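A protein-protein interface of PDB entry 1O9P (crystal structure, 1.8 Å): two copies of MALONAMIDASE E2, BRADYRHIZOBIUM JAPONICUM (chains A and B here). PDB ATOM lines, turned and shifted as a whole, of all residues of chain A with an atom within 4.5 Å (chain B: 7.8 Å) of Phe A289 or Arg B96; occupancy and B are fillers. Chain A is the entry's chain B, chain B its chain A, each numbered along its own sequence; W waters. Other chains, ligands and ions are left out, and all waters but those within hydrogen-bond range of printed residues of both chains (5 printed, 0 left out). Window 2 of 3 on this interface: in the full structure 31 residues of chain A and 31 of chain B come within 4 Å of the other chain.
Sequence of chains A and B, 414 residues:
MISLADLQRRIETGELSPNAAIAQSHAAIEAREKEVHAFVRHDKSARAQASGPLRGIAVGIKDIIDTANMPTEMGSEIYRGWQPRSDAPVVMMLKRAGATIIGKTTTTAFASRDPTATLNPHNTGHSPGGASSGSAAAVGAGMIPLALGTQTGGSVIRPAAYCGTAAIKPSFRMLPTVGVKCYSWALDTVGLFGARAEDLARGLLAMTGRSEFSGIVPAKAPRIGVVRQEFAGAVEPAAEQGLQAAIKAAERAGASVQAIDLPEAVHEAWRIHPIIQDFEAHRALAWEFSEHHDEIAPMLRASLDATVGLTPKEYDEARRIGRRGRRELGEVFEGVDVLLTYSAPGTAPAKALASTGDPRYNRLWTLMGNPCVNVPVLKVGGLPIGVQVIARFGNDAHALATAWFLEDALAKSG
Among the printed residues, pairs that only touch across the chains: His A282 with Arg B96 (3.97 Å), Arg A283 with Pro B89 (3.3 Å), Arg A283 with Met B93 (3.5 Å), Ala A286 with Met B92 (3.5 Å), Trp A287 with Met B92 (3.5 Å), Phe A289 with Arg B96 (3.7 Å) and Ser A290 with Met B92 (3.6 Å).
Of chain B, only Arg B96 (3.7 Å) comes within 4 Å of Phe A289. Of the printed residues of chain A, Arg B96 touches His A282, Ala A286, Phe A289 and Ser A290. Of the printed residues of chain B, Ala A286 touches Met B92 (3.5 Å) and Arg B96 (3.2 Å). Of the printed residues of chain B, Ser A290 touches Met B92 (3.6 Å) and Arg B96 (2.8 Å). The nearest printed residue of chain A that does not touch Met B92 is Glu A291 (4.5 Å).
Of the 18 printed residues of chain B, 5 touch a printed residue of chain A. Printed residues of chain B that touch a printed residue of chain A: Pro B89, Met B92, Met B93, Lys B95 and Arg B96. Along chain B the printed residues that touch a printed residue of chain A span positions 89 to 96. Of the 14 printed residues of chain A, 7 touch a printed residue of chain B. Printed residues of chain A that touch a printed residue of chain B: His A282, Arg A283, Ala A286, Trp A287, Phe A289, Ser A290 and Glu A291. Hydrophobic or aromatic side chains of chain A within 4 Å of the printed part of chain B: Ala A286, Trp A287 and Phe A289.
NZ of Lys B95 is in salt-bridge range of OE1 of Glu A291. NH2 of Arg B96 is in hydrogen-bond range of O of Ala A286, at 3.2 Å. OG of Ser A290 sits at hydrogen-bond distance from NH2 of Arg B96 (2.8 Å).
Water W1 lies within hydrogen-bond range of the backbone carbonyl oxygen of His A282 (2.7 Å) and the guanidinium group of Arg B96 (2.9 Å). Water W5 lies within hydrogen-bond range of the backbone carbonyl oxygen (O) of Arg A283 (2.9 Å) and the backbone carbonyl oxygen (O) of Pro B89 (3.1 Å). Water W2 lies within hydrogen-bond range of ND1 of His A282 and NH1 of Arg B96. Water W4 bridges the guanidinium group of Arg B96 (3.0 Å) and the guanidinium group of Arg A283 (3.4 Å). Water W3 bridges NH1 of Arg A283 (3.5 Å) and NH1 of Arg B96 (3.5 Å).
No position is printed for both chains. Of the 10 pairs that touch across the chains among the printed residues, none has its exchanged pair printed and touching as well.
NE2 of Gln B49 is in hydrogen-bond range of O of Lys B95. O of Leu A304 lies within hydrogen-bond range of NE2 of His A282. A ring nitrogen (NE2) of His A282 is in hydrogen-bond range of the backbone NH of Val A308 (3.3 Å). The backbone carbonyl oxygen of Ala A286 lies within hydrogen-bond range of the side-chain hydroxyl of Ser A290, at 3.2 Å.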
ATOM      1  N   HIS A 282      -7.872  16.270 -18.553  1.00  0.00           N
ATOM      2  CA  HIS A 282      -7.338  15.035 -19.123  1.00  0.00           C
ATOM      3  C   HIS A 282      -5.870  15.173 -19.492  1.00  0.00           C
ATOM      4  O   HIS A 282      -5.114  14.205 -19.444  1.00  0.00           O
ATOM      5  CB  HIS A 282      -8.150  14.615 -20.348  1.00  0.00           C
ATOM      6  CG  HIS A 282      -9.265  13.672 -20.026  1.00  0.00           C
ATOM      7  ND1 HIS A 282      -9.046  12.363 -19.650  1.00  0.00           N
ATOM      8  CD2 HIS A 282     -10.606  13.856 -19.982  1.00  0.00           C
ATOM      9  CE1 HIS A 282     -10.202  11.782 -19.389  1.00  0.00           C
ATOM     10  NE2 HIS A 282     -11.165  12.666 -19.582  1.00  0.00           N
ATOM     11  N   ARG A 283      -5.464  16.377 -19.869  1.00  0.00           N
ATOM     12  CA  ARG A 283      -4.066  16.603 -20.204  1.00  0.00           C
ATOM     13  C   ARG A 283      -3.274  16.804 -18.913  1.00  0.00           C
ATOM     14  O   ARG A 283      -2.205  16.219 -18.728  1.00  0.00           O
ATOM     15  CB  ARG A 283      -3.929  17.837 -21.105  1.00  0.00           C
ATOM     16  CG  ARG A 283      -3.514  17.519 -22.535  1.00  0.00           C
ATOM     17  CD  ARG A 283      -4.333  16.376 -23.118  1.00  0.00           C
ATOM     18  NE  ARG A 283      -5.751  16.698 -23.161  1.00  0.00           N
ATOM     19  CZ  ARG A 283      -6.717  15.818 -23.401  1.00  0.00           C
ATOM     20  NH1 ARG A 283      -6.433  14.539 -23.626  1.00  0.00           N
ATOM     21  NH2 ARG A 283      -7.975  16.224 -23.416  1.00  0.00           N
ATOM     22  N   LEU A 285      -3.866  15.757 -15.933  1.00  0.00           N
ATOM     23  CA  LEU A 285      -3.789  14.566 -15.090  1.00  0.00           C
ATOM     24  C   LEU A 285      -3.538  13.316 -15.926  1.00  0.00           C
ATOM     25  O   LEU A 285      -3.942  12.214 -15.549  1.00  0.00           O
ATOM     26  CB  LEU A 285      -5.085  14.407 -14.297  1.00  0.00           C
ATOM     27  CG  LEU A 285      -5.395  15.517 -13.293  1.00  0.00           C
ATOM     28  CD1 LEU A 285      -6.809  15.340 -12.752  1.00  0.00           C
ATOM     29  CD2 LEU A 285      -4.374  15.479 -12.162  1.00  0.00           C
ATOM     30  N   ALA A 286      -2.855  13.488 -17.057  1.00  0.00           N
ATOM     31  CA  ALA A 286      -2.570  12.371 -17.952  1.00  0.00           C
ATOM     32  C   ALA A 286      -1.828  11.214 -17.284  1.00  0.00           C
ATOM     33  O   ALA A 286      -2.206  10.055 -17.444  1.00  0.00           O
ATOM     34  CB  ALA A 286      -1.789  12.858 -19.162  1.00  0.00           C
ATOM     35  N   TRP A 287      -0.771  11.522 -16.543  1.00  0.00           N
ATOM     36  CA  TRP A 287       0.001  10.484 -15.872  1.00  0.00           C
ATOM     37  C   TRP A 287      -0.874   9.696 -14.891  1.00  0.00           C
ATOM     38  O   TRP A 287      -0.827   8.466 -14.850  1.00  0.00           O
ATOM     39  CB  TRP A 287       1.180  11.111 -15.124  1.00  0.00           C
ATOM     40  CG  TRP A 287       2.010  10.118 -14.365  1.00  0.00           C
ATOM     41  CD1 TRP A 287       2.966   9.276 -14.872  1.00  0.00           C
ATOM     42  CD2 TRP A 287       1.936   9.845 -12.965  1.00  0.00           C
ATOM     43  NE1 TRP A 287       3.491   8.500 -13.867  1.00  0.00           N
ATOM     44  CE2 TRP A 287       2.876   8.827 -12.687  1.00  0.00           C
ATOM     45  CE3 TRP A 287       1.164  10.363 -11.914  1.00  0.00           C
ATOM     46  CZ2 TRP A 287       3.065   8.316 -11.397  1.00  0.00           C
ATOM     47  CZ3 TRP A 287       1.352   9.856 -10.633  1.00  0.00           C
ATOM     48  CH2 TRP A 287       2.297   8.841 -10.386  1.00  0.00           C
ATOM     49  N   GLU A 288      -1.677  10.408 -14.109  1.00  0.00           N
ATOM     50  CA  GLU A 288      -2.552   9.762 -13.135  1.00  0.00           C
ATOM     51  C   GLU A 288      -3.620   8.888 -13.790  1.00  0.00           C
ATOM     52  O   GLU A 288      -3.859   7.758 -13.367  1.00  0.00           O
ATOM     53  CB  GLU A 288      -3.231  10.812 -12.252  1.00  0.00           C
ATOM     54  CG  GLU A 288      -2.282  11.526 -11.291  1.00  0.00           C
ATOM     55  CD  GLU A 288      -1.622  12.759 -11.883  1.00  0.00           C
ATOM     56  OE1 GLU A 288      -1.673  12.948 -13.116  1.00  0.00           O
ATOM     57  OE2 GLU A 288      -1.037  13.543 -11.101  1.00  0.00           O
ATOM     58  N   PHE A 289      -4.255   9.420 -14.827  1.00  0.00           N
ATOM     59  CA  PHE A 289      -5.314   8.706 -15.534  1.00  0.00           C
ATOM     60  C   PHE A 289      -4.792   7.475 -16.285  1.00  0.00           C
ATOM     61  O   PHE A 289      -5.474   6.448 -16.350  1.00  0.00           O
ATOM     62  CB  PHE A 289      -6.004   9.664 -16.513  1.00  0.00           C
ATOM     63  CG  PHE A 289      -7.263   9.110 -17.129  1.00  0.00           C
ATOM     64  CD1 PHE A 289      -8.431   9.002 -16.384  1.00  0.00           C
ATOM     65  CD2 PHE A 289      -7.275   8.696 -18.458  1.00  0.00           C
ATOM     66  CE1 PHE A 289      -9.604   8.486 -16.954  1.00  0.00           C
ATOM     67  CE2 PHE A 289      -8.436   8.181 -19.039  1.00  0.00           C
ATOM     68  CZ  PHE A 289      -9.604   8.076 -18.282  1.00  0.00           C
ATOM     69  N   SER A 290      -3.585   7.580 -16.839  1.00  0.00           N
ATOM     70  CA  SER A 290      -2.985   6.484 -17.601  1.00  0.00           C
ATOM     71  C   SER A 290      -2.290   5.403 -16.772  1.00  0.00           C
ATOM     72  O   SER A 290      -2.413   4.217 -17.074  1.00  0.00           O
ATOM     73  CB  SER A 290      -1.966   7.030 -18.613  1.00  0.00           C
ATOM     74  OG  SER A 290      -2.581   7.808 -19.626  1.00  0.00           O
ATOM     75  N   GLU A 291      -1.567   5.814 -15.735  1.00  0.00           N
ATOM     76  CA  GLU A 291      -0.806   4.879 -14.905  1.00  0.00           C
ATOM     77  C   GLU A 291      -1.415   4.512 -13.557  1.00  0.00           C
ATOM     78  O   GLU A 291      -1.008   3.525 -12.943  1.00  0.00           O
ATOM     79  CB  GLU A 291       0.592   5.444 -14.640  1.00  0.00           C
ATOM     80  CG  GLU A 291       1.273   6.071 -15.835  1.00  0.00           C
ATOM     81  CD  GLU A 291       1.991   5.064 -16.695  1.00  0.00           C
ATOM     82  OE1 GLU A 291       2.757   5.492 -17.587  1.00  0.00           O
ATOM     83  OE2 GLU A 291       1.787   3.849 -16.482  1.00  0.00           O
ATOM     84  N   HIS A 293      -5.106   4.894 -12.920  1.00  0.00           N
ATOM     85  CA  HIS A 293      -6.532   5.089 -13.138  1.00  0.00           C
ATOM     86  C   HIS A 293      -7.435   4.670 -11.984  1.00  0.00           C
ATOM     87  O   HIS A 293      -8.215   5.479 -11.484  1.00  0.00           O
ATOM     88  CB  HIS A 293      -6.959   4.360 -14.416  1.00  0.00           C
ATOM     89  CG  HIS A 293      -8.415   4.500 -14.736  1.00  0.00           C
ATOM     90  ND1 HIS A 293      -9.387   3.737 -14.126  1.00  0.00           N
ATOM     91  CD2 HIS A 293      -9.065   5.332 -15.584  1.00  0.00           C
ATOM     92  CE1 HIS A 293     -10.574   4.092 -14.584  1.00  0.00           C
ATOM     93  NE2 HIS A 293     -10.407   5.058 -15.471  1.00  0.00           N
ATOM     94  N   ILE A 296      -7.495   6.767  -8.656  1.00  0.00           N
ATOM     95  CA  ILE A 296      -8.081   8.102  -8.607  1.00  0.00           C
ATOM     96  C   ILE A 296      -9.411   7.984  -7.864  1.00  0.00           C
ATOM     97  O   ILE A 296     -10.135   7.002  -8.043  1.00  0.00           O
ATOM     98  CB  ILE A 296      -8.326   8.650 -10.036  1.00  0.00           C
ATOM     99  CG1 ILE A 296      -6.994   8.739 -10.789  1.00  0.00           C
ATOM    100  CG2 ILE A 296      -8.968  10.030  -9.968  1.00  0.00           C
ATOM    101  CD1 ILE A 296      -7.129   9.182 -12.234  1.00  0.00           C
ATOM    102  N   LEU A 304     -13.746  11.881 -15.352  1.00  0.00           N
ATOM    103  CA  LEU A 304     -12.697  11.779 -16.362  1.00  0.00           C
ATOM    104  C   LEU A 304     -13.077  10.712 -17.386  1.00  0.00           C
ATOM    105  O   LEU A 304     -12.963  10.926 -18.590  1.00  0.00           O
ATOM    106  CB  LEU A 304     -11.357  11.410 -15.715  1.00  0.00           C
ATOM    107  CG  LEU A 304     -10.708  12.496 -14.856  1.00  0.00           C
ATOM    108  CD1 LEU A 304      -9.435  11.961 -14.210  1.00  0.00           C
ATOM    109  CD2 LEU A 304     -10.402  13.709 -15.725  1.00  0.00           C
ATOM    110  N   ASP A 305     -13.531   9.563 -16.899  1.00  0.00           N
ATOM    111  CA  ASP A 305     -13.929   8.470 -17.781  1.00  0.00           C
ATOM    112  C   ASP A 305     -15.007   8.905 -18.770  1.00  0.00           C
ATOM    113  O   ASP A 305     -15.018   8.469 -19.921  1.00  0.00           O
ATOM    114  CB  ASP A 305     -14.445   7.287 -16.956  1.00  0.00           C
ATOM    115  CG  ASP A 305     -13.324   6.424 -16.401  1.00  0.00           C
ATOM    116  OD1 ASP A 305     -13.613   5.528 -15.580  1.00  0.00           O
ATOM    117  OD2 ASP A 305     -12.156   6.634 -16.797  1.00  0.00           O
ATOM    118  N   VAL A 308     -13.345  11.473 -21.755  1.00  0.00           N
ATOM    119  CA  VAL A 308     -12.175  11.092 -22.539  1.00  0.00           C
ATOM    120  C   VAL A 308     -12.297  11.523 -24.004  1.00  0.00           C
ATOM    121  O   VAL A 308     -11.300  11.872 -24.643  1.00  0.00           O
ATOM    122  CB  VAL A 308     -11.961   9.565 -22.499  1.00  0.00           C
ATOM    123  CG1 VAL A 308     -10.744   9.183 -23.333  1.00  0.00           C
ATOM    124  CG2 VAL A 308     -11.788   9.104 -21.066  1.00  0.00           C
ATOM    125  N   GLN B  49       7.651   1.223 -28.062  1.00  0.00           N
ATOM    126  CA  GLN B  49       6.345   0.786 -27.590  1.00  0.00           C
ATOM    127  C   GLN B  49       5.691   0.000 -28.717  1.00  0.00           C
ATOM    128  O   GLN B  49       6.132   0.068 -29.865  1.00  0.00           O
ATOM    129  CB  GLN B  49       5.473   1.978 -27.184  1.00  0.00           C
ATOM    130  CG  GLN B  49       6.007   2.738 -25.980  1.00  0.00           C
ATOM    131  CD  GLN B  49       4.938   3.569 -25.293  1.00  0.00           C
ATOM    132  OE1 GLN B  49       3.968   3.031 -24.762  1.00  0.00           O
ATOM    133  NE2 GLN B  49       5.111   4.886 -25.304  1.00  0.00           N
ATOM    134  N   SER B  51       2.406   0.202 -30.009  1.00  0.00           N
ATOM    135  CA  SER B  51       1.511   0.877 -30.949  1.00  0.00           C
ATOM    136  C   SER B  51       1.544   2.394 -30.840  1.00  0.00           C
ATOM    137  O   SER B  51       2.117   2.947 -29.904  1.00  0.00           O
ATOM    138  CB  SER B  51       0.075   0.402 -30.731  1.00  0.00           C
ATOM    139  OG  SER B  51      -0.439   0.900 -29.506  1.00  0.00           O
ATOM    140  N   GLY B  52       0.909   3.057 -31.801  1.00  0.00           N
ATOM    141  CA  GLY B  52       0.868   4.509 -31.799  1.00  0.00           C
ATOM    142  C   GLY B  52       1.700   5.095 -32.923  1.00  0.00           C
ATOM    143  O   GLY B  52       2.664   4.467 -33.361  1.00  0.00           O
ATOM    144  N   PRO B  53       1.362   6.301 -33.404  1.00  0.00           N
ATOM    145  CA  PRO B  53       2.114   6.938 -34.492  1.00  0.00           C
ATOM    146  C   PRO B  53       3.581   7.217 -34.174  1.00  0.00           C
ATOM    147  O   PRO B  53       4.400   7.372 -35.084  1.00  0.00           O
ATOM    148  CB  PRO B  53       1.316   8.211 -34.764  1.00  0.00           C
ATOM    149  CG  PRO B  53       0.721   8.534 -33.424  1.00  0.00           C
ATOM    150  CD  PRO B  53       0.266   7.173 -32.945  1.00  0.00           C
ATOM    151  N   LEU B  54       3.917   7.281 -32.890  1.00  0.00           N
ATOM    152  CA  LEU B  54       5.297   7.534 -32.504  1.00  0.00           C
ATOM    153  C   LEU B  54       6.036   6.291 -32.030  1.00  0.00           C
ATOM    154  O   LEU B  54       7.111   6.388 -31.448  1.00  0.00           O
ATOM    155  CB  LEU B  54       5.361   8.626 -31.427  1.00  0.00           C
ATOM    156  CG  LEU B  54       4.889  10.006 -31.897  1.00  0.00           C
ATOM    157  CD1 LEU B  54       5.084  11.028 -30.780  1.00  0.00           C
ATOM    158  CD2 LEU B  54       5.672  10.416 -33.140  1.00  0.00           C
ATOM    159  N   PRO B  89       2.671  16.581 -18.397  1.00  0.00           N
ATOM    160  CA  PRO B  89       1.668  16.350 -19.435  1.00  0.00           C
ATOM    161  C   PRO B  89       2.247  16.228 -20.852  1.00  0.00           C
ATOM    162  O   PRO B  89       1.822  15.364 -21.611  1.00  0.00           O
ATOM    163  CB  PRO B  89       0.741  17.544 -19.268  1.00  0.00           C
ATOM    164  CG  PRO B  89       0.696  17.673 -17.776  1.00  0.00           C
ATOM    165  CD  PRO B  89       2.166  17.524 -17.384  1.00  0.00           C
ATOM    166  N   VAL B  90       3.214  17.071 -21.219  1.00  0.00           N
ATOM    167  CA  VAL B  90       3.784  16.964 -22.566  1.00  0.00           C
ATOM    168  C   VAL B  90       4.527  15.651 -22.751  1.00  0.00           C
ATOM    169  O   VAL B  90       4.608  15.132 -23.862  1.00  0.00           O
ATOM    170  CB  VAL B  90       4.742  18.134 -22.915  1.00  0.00           C
ATOM    171  CG1 VAL B  90       3.938  19.397 -23.171  1.00  0.00           C
ATOM    172  CG2 VAL B  90       5.744  18.350 -21.798  1.00  0.00           C
ATOM    173  N   VAL B  91       5.076  15.111 -21.668  1.00  0.00           N
ATOM    174  CA  VAL B  91       5.766  13.833 -21.755  1.00  0.00           C
ATOM    175  C   VAL B  91       4.705  12.758 -21.985  1.00  0.00           C
ATOM    176  O   VAL B  91       4.913  11.832 -22.767  1.00  0.00           O
ATOM    177  CB  VAL B  91       6.544  13.510 -20.462  1.00  0.00           C
ATOM    178  CG1 VAL B  91       7.090  12.077 -20.522  1.00  0.00           C
ATOM    179  CG2 VAL B  91       7.692  14.498 -20.288  1.00  0.00           C
ATOM    180  N   MET B  92       3.563  12.889 -21.312  1.00  0.00           N
ATOM    181  CA  MET B  92       2.482  11.919 -21.470  1.00  0.00           C
ATOM    182  C   MET B  92       1.881  11.978 -22.872  1.00  0.00           C
ATOM    183  O   MET B  92       1.435  10.958 -23.393  1.00  0.00           O
ATOM    184  CB  MET B  92       1.375  12.148 -20.432  1.00  0.00           C
ATOM    185  CG  MET B  92       1.744  11.749 -19.005  1.00  0.00           C
ATOM    186  SD  MET B  92       2.319  10.038 -18.843  1.00  0.00           S
ATOM    187  CE  MET B  92       0.847   9.105 -19.413  1.00  0.00           C
ATOM    188  N   MET B  93       1.859  13.162 -23.483  1.00  0.00           N
ATOM    189  CA  MET B  93       1.318  13.279 -24.837  1.00  0.00           C
ATOM    190  C   MET B  93       2.190  12.422 -25.754  1.00  0.00           C
ATOM    191  O   MET B  93       1.694  11.744 -26.650  1.00  0.00           O
ATOM    192  CB  MET B  93       1.335  14.737 -25.322  1.00  0.00           C
ATOM    193  CG  MET B  93       0.475  15.685 -24.491  1.00  0.00           C
ATOM    194  SD  MET B  93       0.550  17.388 -25.095  1.00  0.00           S
ATOM    195  CE  MET B  93      -1.193  17.835 -25.131  1.00  0.00           C
ATOM    196  N   LEU B  94       3.498  12.456 -25.519  1.00  0.00           N
ATOM    197  CA  LEU B  94       4.424  11.663 -26.315  1.00  0.00           C
ATOM    198  C   LEU B  94       4.246  10.171 -26.033  1.00  0.00           C
ATOM    199  O   LEU B  94       4.140   9.365 -26.960  1.00  0.00           O
ATOM    200  CB  LEU B  94       5.866  12.076 -26.014  1.00  0.00           C
ATOM    201  CG  LEU B  94       6.236  13.494 -26.457  1.00  0.00           C
ATOM    202  CD1 LEU B  94       7.606  13.866 -25.910  1.00  0.00           C
ATOM    203  CD2 LEU B  94       6.208  13.571 -27.977  1.00  0.00           C
ATOM    204  N   LYS B  95       4.203   9.811 -24.753  1.00  0.00           N
ATOM    205  CA  LYS B  95       4.058   8.415 -24.353  1.00  0.00           C
ATOM    206  C   LYS B  95       2.746   7.800 -24.828  1.00  0.00           C
ATOM    207  O   LYS B  95       2.715   6.654 -25.273  1.00  0.00           O
ATOM    208  CB  LYS B  95       4.161   8.274 -22.830  1.00  0.00           C
ATOM    209  CG  LYS B  95       5.448   8.831 -22.237  1.00  0.00           C
ATOM    210  CD  LYS B  95       5.843   8.125 -20.937  1.00  0.00           C
ATOM    211  CE  LYS B  95       4.651   7.856 -20.030  1.00  0.00           C
ATOM    212  NZ  LYS B  95       5.043   7.101 -18.803  1.00  0.00           N
ATOM    213  N   ARG B  96       1.664   8.560 -24.734  1.00  0.00           N
ATOM    214  CA  ARG B  96       0.364   8.058 -25.164  1.00  0.00           C
ATOM    215  C   ARG B  96       0.353   7.807 -26.661  1.00  0.00           C
ATOM    216  O   ARG B  96      -0.432   6.994 -27.157  1.00  0.00           O
ATOM    217  CB  ARG B  96      -0.737   9.052 -24.799  1.00  0.00           C
ATOM    218  CG  ARG B  96      -1.024   9.107 -23.310  1.00  0.00           C
ATOM    219  CD  ARG B  96      -2.172  10.053 -23.010  1.00  0.00           C
ATOM    220  NE  ARG B  96      -2.691   9.834 -21.663  1.00  0.00           N
ATOM    221  CZ  ARG B  96      -3.807  10.378 -21.193  1.00  0.00           C
ATOM    222  NH1 ARG B  96      -4.526  11.188 -21.962  1.00  0.00           N
ATOM    223  NH2 ARG B  96      -4.217  10.084 -19.964  1.00  0.00           N
ATOM    224  N   ALA B  97       1.229   8.507 -27.375  1.00  0.00           N
ATOM    225  CA  ALA B  97       1.325   8.367 -28.821  1.00  0.00           C
ATOM    226  C   ALA B  97       2.269   7.238 -29.225  1.00  0.00           C
ATOM    227  O   ALA B  97       2.450   6.972 -30.414  1.00  0.00           O
ATOM    228  CB  ALA B  97       1.780   9.687 -29.443  1.00  0.00           C
ATOM    229  N   GLY B  98       2.880   6.588 -28.234  1.00  0.00           N
ATOM    230  CA  GLY B  98       3.779   5.476 -28.508  1.00  0.00           C
ATOM    231  C   GLY B  98       5.269   5.771 -28.551  1.00  0.00           C
ATOM    232  O   GLY B  98       6.067   4.892 -28.893  1.00  0.00           O
ATOM    233  N   ALA B  99       5.660   6.989 -28.191  1.00  0.00           N
ATOM    234  CA  ALA B  99       7.071   7.368 -28.218  1.00  0.00           C
ATOM    235  C   ALA B  99       7.896   6.743 -27.095  1.00  0.00           C
ATOM    236  O   ALA B  99       7.358   6.265 -26.098  1.00  0.00           O
ATOM    237  CB  ALA B  99       7.199   8.892 -28.166  1.00  0.00           C
ATOM    238  N   ALA B 206       0.788  13.983 -33.458  1.00  0.00           N
ATOM    239  CA  ALA B 206       0.767  12.868 -32.519  1.00  0.00           C
ATOM    240  C   ALA B 206       0.527  13.333 -31.088  1.00  0.00           C
ATOM    241  O   ALA B 206      -0.232  12.709 -30.342  1.00  0.00           O
ATOM    242  CB  ALA B 206       2.087  12.093 -32.599  1.00  0.00           C
ATOM    243  N   MET B 207       1.168  14.434 -30.709  1.00  0.00           N
ATOM    244  CA  MET B 207       1.024  14.959 -29.357  1.00  0.00           C
ATOM    245  C   MET B 207      -0.337  15.567 -29.042  1.00  0.00           C
ATOM    246  O   MET B 207      -0.859  15.372 -27.944  1.00  0.00           O
ATOM    247  CB  MET B 207       2.089  16.020 -29.078  1.00  0.00           C
ATOM    248  CG  MET B 207       3.508  15.495 -28.945  1.00  0.00           C
ATOM    249  SD  MET B 207       4.684  16.857 -28.693  1.00  0.00           S
ATOM    250  CE  MET B 207       4.367  17.290 -26.984  1.00  0.00           C
HETATM  251  O   HOH W   1      -6.265  11.803 -18.858  1.00  0.00           O
HETATM  252  O   HOH W   2      -7.524  11.045 -21.862  1.00  0.00           O
HETATM  253  O   HOH W   3      -3.037  13.965 -23.404  1.00  0.00           O
HETATM  254  O   HOH W   4      -4.699  11.867 -24.922  1.00  0.00           O
HETATM  255  O   HOH W   5      -1.232  15.397 -21.339  1.00  0.00           O
